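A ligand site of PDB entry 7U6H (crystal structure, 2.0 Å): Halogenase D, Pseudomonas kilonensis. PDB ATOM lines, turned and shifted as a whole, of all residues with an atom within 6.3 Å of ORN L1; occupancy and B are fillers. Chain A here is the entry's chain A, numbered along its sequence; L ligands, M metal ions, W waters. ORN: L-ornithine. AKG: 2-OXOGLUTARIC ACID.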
ATOM      1  N   VAL A  79     -11.069 -15.256 -12.340  1.00  0.00           N
ATOM      2  CA  VAL A  79     -10.055 -15.618 -11.359  1.00  0.00           C
ATOM      3  C   VAL A  79      -8.938 -16.365 -12.095  1.00  0.00           C
ATOM      4  O   VAL A  79      -9.117 -17.540 -12.460  1.00  0.00           O
ATOM      5  CB  VAL A  79     -10.633 -16.461 -10.213  1.00  0.00           C
ATOM      6  CG1 VAL A  79      -9.535 -16.880  -9.257  1.00  0.00           C
ATOM      7  CG2 VAL A  79     -11.695 -15.668  -9.486  1.00  0.00           C
ATOM      8  N   SER A  81      -6.299 -17.797 -11.097  1.00  0.00           N
ATOM      9  CA  SER A  81      -5.819 -18.991 -10.407  1.00  0.00           C
ATOM     10  C   SER A  81      -6.762 -20.179 -10.547  1.00  0.00           C
ATOM     11  O   SER A  81      -6.375 -21.306 -10.200  1.00  0.00           O
ATOM     12  CB  SER A  81      -5.582 -18.696  -8.924  1.00  0.00           C
ATOM     13  OG  SER A  81      -6.772 -18.277  -8.279  1.00  0.00           O
ATOM     14  N   THR A  82      -7.987 -19.969 -11.037  1.00  0.00           N
ATOM     15  CA  THR A  82      -8.909 -21.075 -11.278  1.00  0.00           C
ATOM     16  C   THR A  82      -9.269 -21.186 -12.746  1.00  0.00           C
ATOM     17  O   THR A  82     -10.440 -21.322 -13.093  1.00  0.00           O
ATOM     18  CB  THR A  82     -10.188 -20.907 -10.439  1.00  0.00           C
ATOM     19  OG1 THR A  82     -10.867 -19.717 -10.852  1.00  0.00           O
ATOM     20  CG2 THR A  82      -9.858 -20.806  -8.962  1.00  0.00           C
ATOM     21  N   ARG A  87     -16.751 -14.986 -11.761  1.00  0.00           N
ATOM     22  CA  ARG A  87     -17.422 -14.677 -10.505  1.00  0.00           C
ATOM     23  C   ARG A  87     -18.298 -13.460 -10.761  1.00  0.00           C
ATOM     24  O   ARG A  87     -17.792 -12.344 -10.877  1.00  0.00           O
ATOM     25  CB  ARG A  87     -16.437 -14.409  -9.370  1.00  0.00           C
ATOM     26  CG  ARG A  87     -15.309 -15.410  -9.268  1.00  0.00           C
ATOM     27  CD  ARG A  87     -15.733 -16.657  -8.510  1.00  0.00           C
ATOM     28  NE  ARG A  87     -14.594 -17.516  -8.212  1.00  0.00           N
ATOM     29  CZ  ARG A  87     -13.987 -18.300  -9.101  1.00  0.00           C
ATOM     30  NH1 ARG A  87     -14.425 -18.341 -10.355  1.00  0.00           N
ATOM     31  NH2 ARG A  87     -12.949 -19.035  -8.739  1.00  0.00           N
ATOM     32  N   GLU A 132     -10.665 -14.423   5.035  1.00  0.00           N
ATOM     33  CA  GLU A 132     -11.429 -15.489   4.402  1.00  0.00           C
ATOM     34  C   GLU A 132     -12.296 -16.234   5.412  1.00  0.00           C
ATOM     35  O   GLU A 132     -12.939 -17.230   5.045  1.00  0.00           O
ATOM     36  CB  GLU A 132     -10.506 -16.476   3.675  1.00  0.00           C
ATOM     37  CG  GLU A 132     -11.166 -17.184   2.500  1.00  0.00           C
ATOM     38  CD  GLU A 132     -10.302 -18.268   1.889  1.00  0.00           C
ATOM     39  OE1 GLU A 132      -9.063 -18.182   2.024  1.00  0.00           O
ATOM     40  OE2 GLU A 132     -10.857 -19.196   1.277  1.00  0.00           O
ATOM     41  N   LEU A 135     -17.599 -15.096   4.410  1.00  0.00           N
ATOM     42  CA  LEU A 135     -17.925 -14.326   3.225  1.00  0.00           C
ATOM     43  C   LEU A 135     -19.369 -14.599   2.820  1.00  0.00           C
ATOM     44  O   LEU A 135     -19.911 -15.665   3.105  1.00  0.00           O
ATOM     45  CB  LEU A 135     -16.984 -14.644   2.045  1.00  0.00           C
ATOM     46  CG  LEU A 135     -15.476 -14.570   2.299  1.00  0.00           C
ATOM     47  CD1 LEU A 135     -14.705 -15.333   1.233  1.00  0.00           C
ATOM     48  CD2 LEU A 135     -15.013 -13.126   2.373  1.00  0.00           C
ATOM     49  N   HIS A 146     -20.763 -18.699  -9.784  1.00  0.00           N
ATOM     50  CA  HIS A 146     -19.552 -18.877  -8.987  1.00  0.00           C
ATOM     51  C   HIS A 146     -18.808 -20.021  -9.668  1.00  0.00           C
ATOM     52  O   HIS A 146     -19.064 -21.199  -9.371  1.00  0.00           O
ATOM     53  CB  HIS A 146     -19.873 -19.168  -7.525  1.00  0.00           C
ATOM     54  CG  HIS A 146     -18.718 -18.967  -6.598  1.00  0.00           C
ATOM     55  ND1 HIS A 146     -18.866 -18.537  -5.299  1.00  0.00           N
ATOM     56  CD2 HIS A 146     -17.382 -19.146  -6.781  1.00  0.00           C
ATOM     57  CE1 HIS A 146     -17.687 -18.457  -4.724  1.00  0.00           C
ATOM     58  NE2 HIS A 146     -16.766 -18.820  -5.604  1.00  0.00           N
ATOM     59  N   GLY A 147     -17.910 -19.686 -10.583  1.00  0.00           N
ATOM     60  CA  GLY A 147     -17.301 -20.672 -11.468  1.00  0.00           C
ATOM     61  C   GLY A 147     -16.467 -21.700 -10.727  1.00  0.00           C
ATOM     62  O   GLY A 147     -16.242 -21.642  -9.516  1.00  0.00           O
ATOM     63  N   TRP A 148     -15.999 -22.681 -11.505  1.00  0.00           N
ATOM     64  CA  TRP A 148     -15.201 -23.782 -10.975  1.00  0.00           C
ATOM     65  C   TRP A 148     -14.013 -23.265 -10.184  1.00  0.00           C
ATOM     66  O   TRP A 148     -13.302 -22.364 -10.629  1.00  0.00           O
ATOM     67  CB  TRP A 148     -14.705 -24.666 -12.124  1.00  0.00           C
ATOM     68  CG  TRP A 148     -15.736 -25.569 -12.751  1.00  0.00           C
ATOM     69  CD1 TRP A 148     -16.259 -25.454 -14.014  1.00  0.00           C
ATOM     70  CD2 TRP A 148     -16.350 -26.726 -12.172  1.00  0.00           C
ATOM     71  NE1 TRP A 148     -17.155 -26.465 -14.247  1.00  0.00           N
ATOM     72  CE2 TRP A 148     -17.231 -27.261 -13.140  1.00  0.00           C
ATOM     73  CE3 TRP A 148     -16.236 -27.366 -10.941  1.00  0.00           C
ATOM     74  CZ2 TRP A 148     -17.997 -28.403 -12.904  1.00  0.00           C
ATOM     75  CZ3 TRP A 148     -17.005 -28.495 -10.699  1.00  0.00           C
ATOM     76  CH2 TRP A 148     -17.868 -29.006 -11.681  1.00  0.00           C
ATOM     77  N   HIS A 149     -13.804 -23.836  -8.999  1.00  0.00           N
ATOM     78  CA  HIS A 149     -12.731 -23.383  -8.130  1.00  0.00           C
ATOM     79  C   HIS A 149     -12.525 -24.411  -7.026  1.00  0.00           C
ATOM     80  O   HIS A 149     -13.298 -25.348  -6.861  1.00  0.00           O
ATOM     81  CB  HIS A 149     -13.045 -22.016  -7.520  1.00  0.00           C
ATOM     82  CG  HIS A 149     -14.178 -22.043  -6.536  1.00  0.00           C
ATOM     83  ND1 HIS A 149     -15.496 -21.975  -6.912  1.00  0.00           N
ATOM     84  CD2 HIS A 149     -14.177 -22.137  -5.180  1.00  0.00           C
ATOM     85  CE1 HIS A 149     -16.264 -22.019  -5.837  1.00  0.00           C
ATOM     86  NE2 HIS A 149     -15.488 -22.124  -4.774  1.00  0.00           N
ATOM     87  N   TRP A 150     -11.442 -24.206  -6.270  1.00  0.00           N
ATOM     88  CA  TRP A 150     -11.204 -24.859  -4.994  1.00  0.00           C
ATOM     89  C   TRP A 150     -11.087 -23.783  -3.915  1.00  0.00           C
ATOM     90  O   TRP A 150     -11.081 -22.588  -4.197  1.00  0.00           O
ATOM     91  CB  TRP A 150      -9.909 -25.695  -5.007  1.00  0.00           C
ATOM     92  CG  TRP A 150      -9.896 -26.866  -5.929  1.00  0.00           C
ATOM     93  CD1 TRP A 150     -10.166 -28.169  -5.597  1.00  0.00           C
ATOM     94  CD2 TRP A 150      -9.555 -26.878  -7.319  1.00  0.00           C
ATOM     95  NE1 TRP A 150     -10.030 -28.973  -6.698  1.00  0.00           N
ATOM     96  CE2 TRP A 150      -9.654 -28.202  -7.771  1.00  0.00           C
ATOM     97  CE3 TRP A 150      -9.178 -25.875  -8.231  1.00  0.00           C
ATOM     98  CZ2 TRP A 150      -9.397 -28.569  -9.091  1.00  0.00           C
ATOM     99  CZ3 TRP A 150      -8.924 -26.240  -9.537  1.00  0.00           C
ATOM    100  CH2 TRP A 150      -9.029 -27.572  -9.953  1.00  0.00           C
ATOM    101  N   GLY A 151     -10.997 -24.233  -2.669  1.00  0.00           N
ATOM    102  CA  GLY A 151     -10.709 -23.354  -1.563  1.00  0.00           C
ATOM    103  C   GLY A 151      -9.259 -23.501  -1.111  1.00  0.00           C
ATOM    104  O   GLY A 151      -8.657 -24.565  -1.243  1.00  0.00           O
ATOM    105  N   ASP A 152      -8.704 -22.407  -0.585  1.00  0.00           N
ATOM    106  CA  ASP A 152      -7.350 -22.471  -0.041  1.00  0.00           C
ATOM    107  C   ASP A 152      -7.305 -23.243   1.272  1.00  0.00           C
ATOM    108  O   ASP A 152      -6.219 -23.671   1.686  1.00  0.00           O
ATOM    109  CB  ASP A 152      -6.798 -21.055   0.172  1.00  0.00           C
ATOM    110  CG  ASP A 152      -6.352 -20.406  -1.125  1.00  0.00           C
ATOM    111  OD1 ASP A 152      -5.406 -20.940  -1.751  1.00  0.00           O
ATOM    112  OD2 ASP A 152      -6.927 -19.376  -1.508  1.00  0.00           O
ATOM    113  N   THR A 156     -15.130 -25.888   4.933  1.00  0.00           N
ATOM    114  CA  THR A 156     -16.023 -24.800   4.581  1.00  0.00           C
ATOM    115  C   THR A 156     -17.456 -25.199   4.902  1.00  0.00           C
ATOM    116  O   THR A 156     -17.882 -26.319   4.577  1.00  0.00           O
ATOM    117  CB  THR A 156     -15.890 -24.449   3.098  1.00  0.00           C
ATOM    118  OG1 THR A 156     -14.625 -23.826   2.864  1.00  0.00           O
ATOM    119  CG2 THR A 156     -17.002 -23.500   2.663  1.00  0.00           C
ATOM    120  N   TRP A 181      -5.864 -28.196  -5.844  1.00  0.00           N
ATOM    121  CA  TRP A 181      -5.781 -26.912  -6.529  1.00  0.00           C
ATOM    122  C   TRP A 181      -4.332 -26.609  -6.893  1.00  0.00           C
ATOM    123  O   TRP A 181      -3.514 -26.309  -6.011  1.00  0.00           O
ATOM    124  CB  TRP A 181      -6.367 -25.806  -5.640  1.00  0.00           C
ATOM    125  CG  TRP A 181      -6.556 -24.489  -6.324  1.00  0.00           C
ATOM    126  CD1 TRP A 181      -6.343 -24.204  -7.634  1.00  0.00           C
ATOM    127  CD2 TRP A 181      -7.009 -23.275  -5.718  1.00  0.00           C
ATOM    128  NE1 TRP A 181      -6.622 -22.881  -7.887  1.00  0.00           N
ATOM    129  CE2 TRP A 181      -7.038 -22.293  -6.726  1.00  0.00           C
ATOM    130  CE3 TRP A 181      -7.386 -22.912  -4.418  1.00  0.00           C
ATOM    131  CZ2 TRP A 181      -7.433 -20.976  -6.470  1.00  0.00           C
ATOM    132  CZ3 TRP A 181      -7.782 -21.613  -4.175  1.00  0.00           C
ATOM    133  CH2 TRP A 181      -7.792 -20.660  -5.196  1.00  0.00           C
ATOM    134  N   ASN A 232     -20.542 -18.180   3.663  1.00  0.00           N
ATOM    135  CA  ASN A 232     -19.413 -19.103   3.624  1.00  0.00           C
ATOM    136  C   ASN A 232     -18.568 -18.854   4.869  1.00  0.00           C
ATOM    137  O   ASN A 232     -17.956 -17.797   5.003  1.00  0.00           O
ATOM    138  CB  ASN A 232     -18.589 -18.909   2.352  1.00  0.00           C
ATOM    139  CG  ASN A 232     -17.392 -19.858   2.259  1.00  0.00           C
ATOM    140  OD1 ASN A 232     -16.785 -20.231   3.260  1.00  0.00           O
ATOM    141  ND2 ASN A 232     -17.050 -20.243   1.033  1.00  0.00           N
ATOM    142  N   CYS A 234     -15.298 -20.469   6.711  1.00  0.00           N
ATOM    143  CA  CYS A 234     -14.189 -21.316   6.285  1.00  0.00           C
ATOM    144  C   CYS A 234     -13.155 -21.423   7.399  1.00  0.00           C
ATOM    145  O   CYS A 234     -12.682 -20.406   7.916  1.00  0.00           O
ATOM    146  CB  CYS A 234     -13.536 -20.748   5.016  1.00  0.00           C
ATOM    147  SG  CYS A 234     -12.130 -21.689   4.420  1.00  0.00           S
ATOM    148  N   GLU A 248      -5.047 -14.773  -3.725  1.00  0.00           N
ATOM    149  CA  GLU A 248      -5.361 -13.963  -4.906  1.00  0.00           C
ATOM    150  C   GLU A 248      -6.841 -14.035  -5.271  1.00  0.00           C
ATOM    151  O   GLU A 248      -7.389 -13.057  -5.803  1.00  0.00           O
ATOM    152  CB  GLU A 248      -4.491 -14.414  -6.085  1.00  0.00           C
ATOM    153  CG  GLU A 248      -4.913 -15.721  -6.743  1.00  0.00           C
ATOM    154  CD  GLU A 248      -4.779 -16.912  -5.817  1.00  0.00           C
ATOM    155  OE1 GLU A 248      -3.763 -16.996  -5.090  1.00  0.00           O
ATOM    156  OE2 GLU A 248      -5.695 -17.762  -5.797  1.00  0.00           O
ATOM    157  N   SER A 249      -7.502 -15.158  -5.006  1.00  0.00           N
ATOM    158  CA  SER A 249      -8.925 -15.271  -5.354  1.00  0.00           C
ATOM    159  C   SER A 249      -9.776 -14.416  -4.426  1.00  0.00           C
ATOM    160  O   SER A 249     -10.714 -13.746  -4.882  1.00  0.00           O
ATOM    161  CB  SER A 249      -9.362 -16.736  -5.316  1.00  0.00           C
ATOM    162  OG  SER A 249      -9.467 -17.212  -3.994  1.00  0.00           O
ATOM    163  N   ILE A 250      -9.472 -14.412  -3.132  1.00  0.00           N
ATOM    164  CA  ILE A 250     -10.226 -13.590  -2.186  1.00  0.00           C
ATOM    165  C   ILE A 250     -10.004 -12.114  -2.492  1.00  0.00           C
ATOM    166  O   ILE A 250     -10.925 -11.298  -2.378  1.00  0.00           O
ATOM    167  CB  ILE A 250      -9.832 -13.941  -0.746  1.00  0.00           C
ATOM    168  CG1 ILE A 250      -9.956 -15.444  -0.495  1.00  0.00           C
ATOM    169  CG2 ILE A 250     -10.687 -13.163   0.256  1.00  0.00           C
ATOM    170  CD1 ILE A 250     -11.284 -16.026  -0.937  1.00  0.00           C
ATOM    171  N   ILE A 253     -12.197 -11.081  -5.676  1.00  0.00           N
ATOM    172  CA  ILE A 253     -13.649 -11.244  -5.593  1.00  0.00           C
ATOM    173  C   ILE A 253     -14.209 -10.382  -4.463  1.00  0.00           C
ATOM    174  O   ILE A 253     -15.108  -9.561  -4.688  1.00  0.00           O
ATOM    175  CB  ILE A 253     -14.023 -12.723  -5.386  1.00  0.00           C
ATOM    176  CG1 ILE A 253     -13.473 -13.584  -6.527  1.00  0.00           C
ATOM    177  CG2 ILE A 253     -15.544 -12.875  -5.291  1.00  0.00           C
ATOM    178  CD1 ILE A 253     -13.367 -15.044  -6.179  1.00  0.00           C
ATOM    179  N   TRP A 254     -13.700 -10.581  -3.250  1.00  0.00           N
ATOM    180  CA  TRP A 254     -14.236  -9.927  -2.066  1.00  0.00           C
ATOM    181  C   TRP A 254     -13.401  -8.746  -1.569  1.00  0.00           C
ATOM    182  O   TRP A 254     -13.944  -7.895  -0.857  1.00  0.00           O
ATOM    183  CB  TRP A 254     -14.382 -10.924  -0.920  1.00  0.00           C
ATOM    184  CG  TRP A 254     -15.489 -11.911  -1.094  1.00  0.00           C
ATOM    185  CD1 TRP A 254     -16.809 -11.720  -0.792  1.00  0.00           C
ATOM    186  CD2 TRP A 254     -15.379 -13.235  -1.609  1.00  0.00           C
ATOM    187  NE1 TRP A 254     -17.526 -12.854  -1.086  1.00  0.00           N
ATOM    188  CE2 TRP A 254     -16.672 -13.803  -1.592  1.00  0.00           C
ATOM    189  CE3 TRP A 254     -14.315 -14.017  -2.089  1.00  0.00           C
ATOM    190  CZ2 TRP A 254     -16.926 -15.096  -2.032  1.00  0.00           C
ATOM    191  CZ3 TRP A 254     -14.573 -15.297  -2.524  1.00  0.00           C
ATOM    192  CH2 TRP A 254     -15.874 -15.826  -2.493  1.00  0.00           C
HETATM  193  N   ORN L   1     -11.021 -19.595  -3.637  1.00  0.00           N
HETATM  194  CA  ORN L   1     -12.459 -19.510  -3.845  1.00  0.00           C
HETATM  195  CB  ORN L   1     -13.141 -18.710  -2.741  1.00  0.00           C
HETATM  196  CG  ORN L   1     -13.238 -19.505  -1.450  1.00  0.00           C
HETATM  197  CD  ORN L   1     -13.775 -18.648  -0.314  1.00  0.00           C
HETATM  198  NE  ORN L   1     -13.697 -19.219   1.018  1.00  0.00           N
HETATM  199  C   ORN L   1     -12.852 -18.875  -5.218  1.00  0.00           C
HETATM  200  O   ORN L   1     -14.064 -18.548  -5.385  1.00  0.00           O
HETATM  201  OXT ORN L   1     -11.950 -18.727  -6.087  1.00  0.00           O
HETATM  202  C1  AKG L   2     -17.802 -20.490  -1.936  1.00  0.00           C
HETATM  203  O1  AKG L   2     -18.277 -19.555  -1.241  1.00  0.00           O
HETATM  204  O2  AKG L   2     -16.562 -20.715  -1.915  1.00  0.00           O
HETATM  205  C2  AKG L   2     -18.722 -21.351  -2.784  1.00  0.00           C
HETATM  206  O5  AKG L   2     -18.289 -22.248  -3.420  1.00  0.00           O
HETATM  207  C3  AKG L   2     -20.231 -21.064  -2.815  1.00  0.00           C
HETATM  208  C4  AKG L   2     -20.986 -22.384  -2.772  1.00  0.00           C
HETATM  209  C5  AKG L   2     -22.480 -22.132  -2.905  1.00  0.00           C
HETATM  210  O3  AKG L   2     -22.900 -20.991  -3.246  1.00  0.00           O
HETATM  211  O4  AKG L   2     -23.296 -23.062  -2.684  1.00  0.00           O
HETATM  212 NI    NI M   1     -16.218 -22.684  -2.931  1.00  0.00          NI
HETATM  213  O   HOH W   1     -14.865 -17.988   3.207  1.00  0.00           O
HETATM  214  O   HOH W   2     -14.288 -22.066   0.999  1.00  0.00           O
HETATM  215  O   HOH W   3      -9.632 -19.747  -1.095  1.00  0.00           O
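The indole nitrogen of Trp 181 is in hydrogen-bond range of the backbone carbonyl oxygen of Ser 81 (2.8 Å).
The backbone NH (N) of Asn 232 lies within hydrogen-bond range of the backbone carbonyl oxygen (O) of Leu 135, 2.7 Å away.
ND1 of His 149 lies within hydrogen-bond range of O of Gly 147 (2.7 Å).
OG1 of Thr 82 sits at hydrogen-bond distance from NH2 of Arg 87 (3.0 Å).
Water W1 lies within hydrogen-bond range of O of Glu 132 (2.8 Å), NE of ORN L1 (2.8 Å) and OD1 of Asn 232 (3.0 Å).
Water W3 lies within hydrogen-bond range of OE2 of Glu 132, OD2 of Asp 152 and N of ORN L1.
Water W2 lies within hydrogen-bond range of the side-chain hydroxyl (OG1) of Thr 156 (2.6 Å), a nitrogen (NE) of ORN L1 (2.9 Å) and the side-chain amide nitrogen (ND2) of Asn 232 (3.3 Å).
Leu 135 touches ORN L1 (CD1 to CD, 3.8 Å).
CD2 of His 149 touches CA of ORN L1, 3.4 Å away.
Trp 181 touches ORN L1 (CH2 to N, 3.7 Å).
Asn 232 touches ORN L1 (ND2 to NE, 3.5 Å).
Ile 250 touches ORN L1 (CD1 to CD, 3.7 Å).
CD1 of Ile 253 touches O of ORN L1, 3.7 Å away.
Trp 254 touches ORN L1.
Along chain A the residues within 4 Å of ORN L1 span positions 87 to 254.
The side-chain hydroxyl (OG) of Ser 249 sits at hydrogen-bond distance from a nitrogen (N) of ORN L1 (2.9 Å).
The side-chain amide nitrogen (ND2) of Asn 232 is in hydrogen-bond range of an oxygen (O1) of AKG L2 (2.7 Å).
A nitrogen (N) of ORN L1 sits at hydrogen-bond distance from the backbone carbonyl oxygen (O) of Trp 150, at 3.0 Å.
The guanidinium group (NH2) of Arg 87 lies within salt-bridge range of an oxygen (OXT) of ORN L1, 2.9 Å away.
The side-chain carboxylate (OE2) of Glu 132 lies within salt-bridge range of a nitrogen (NE) of ORN L1 (2.9 Å).
O of ORN L1 sits at hydrogen-bond distance from NE2 of His 146 (2.7 Å).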
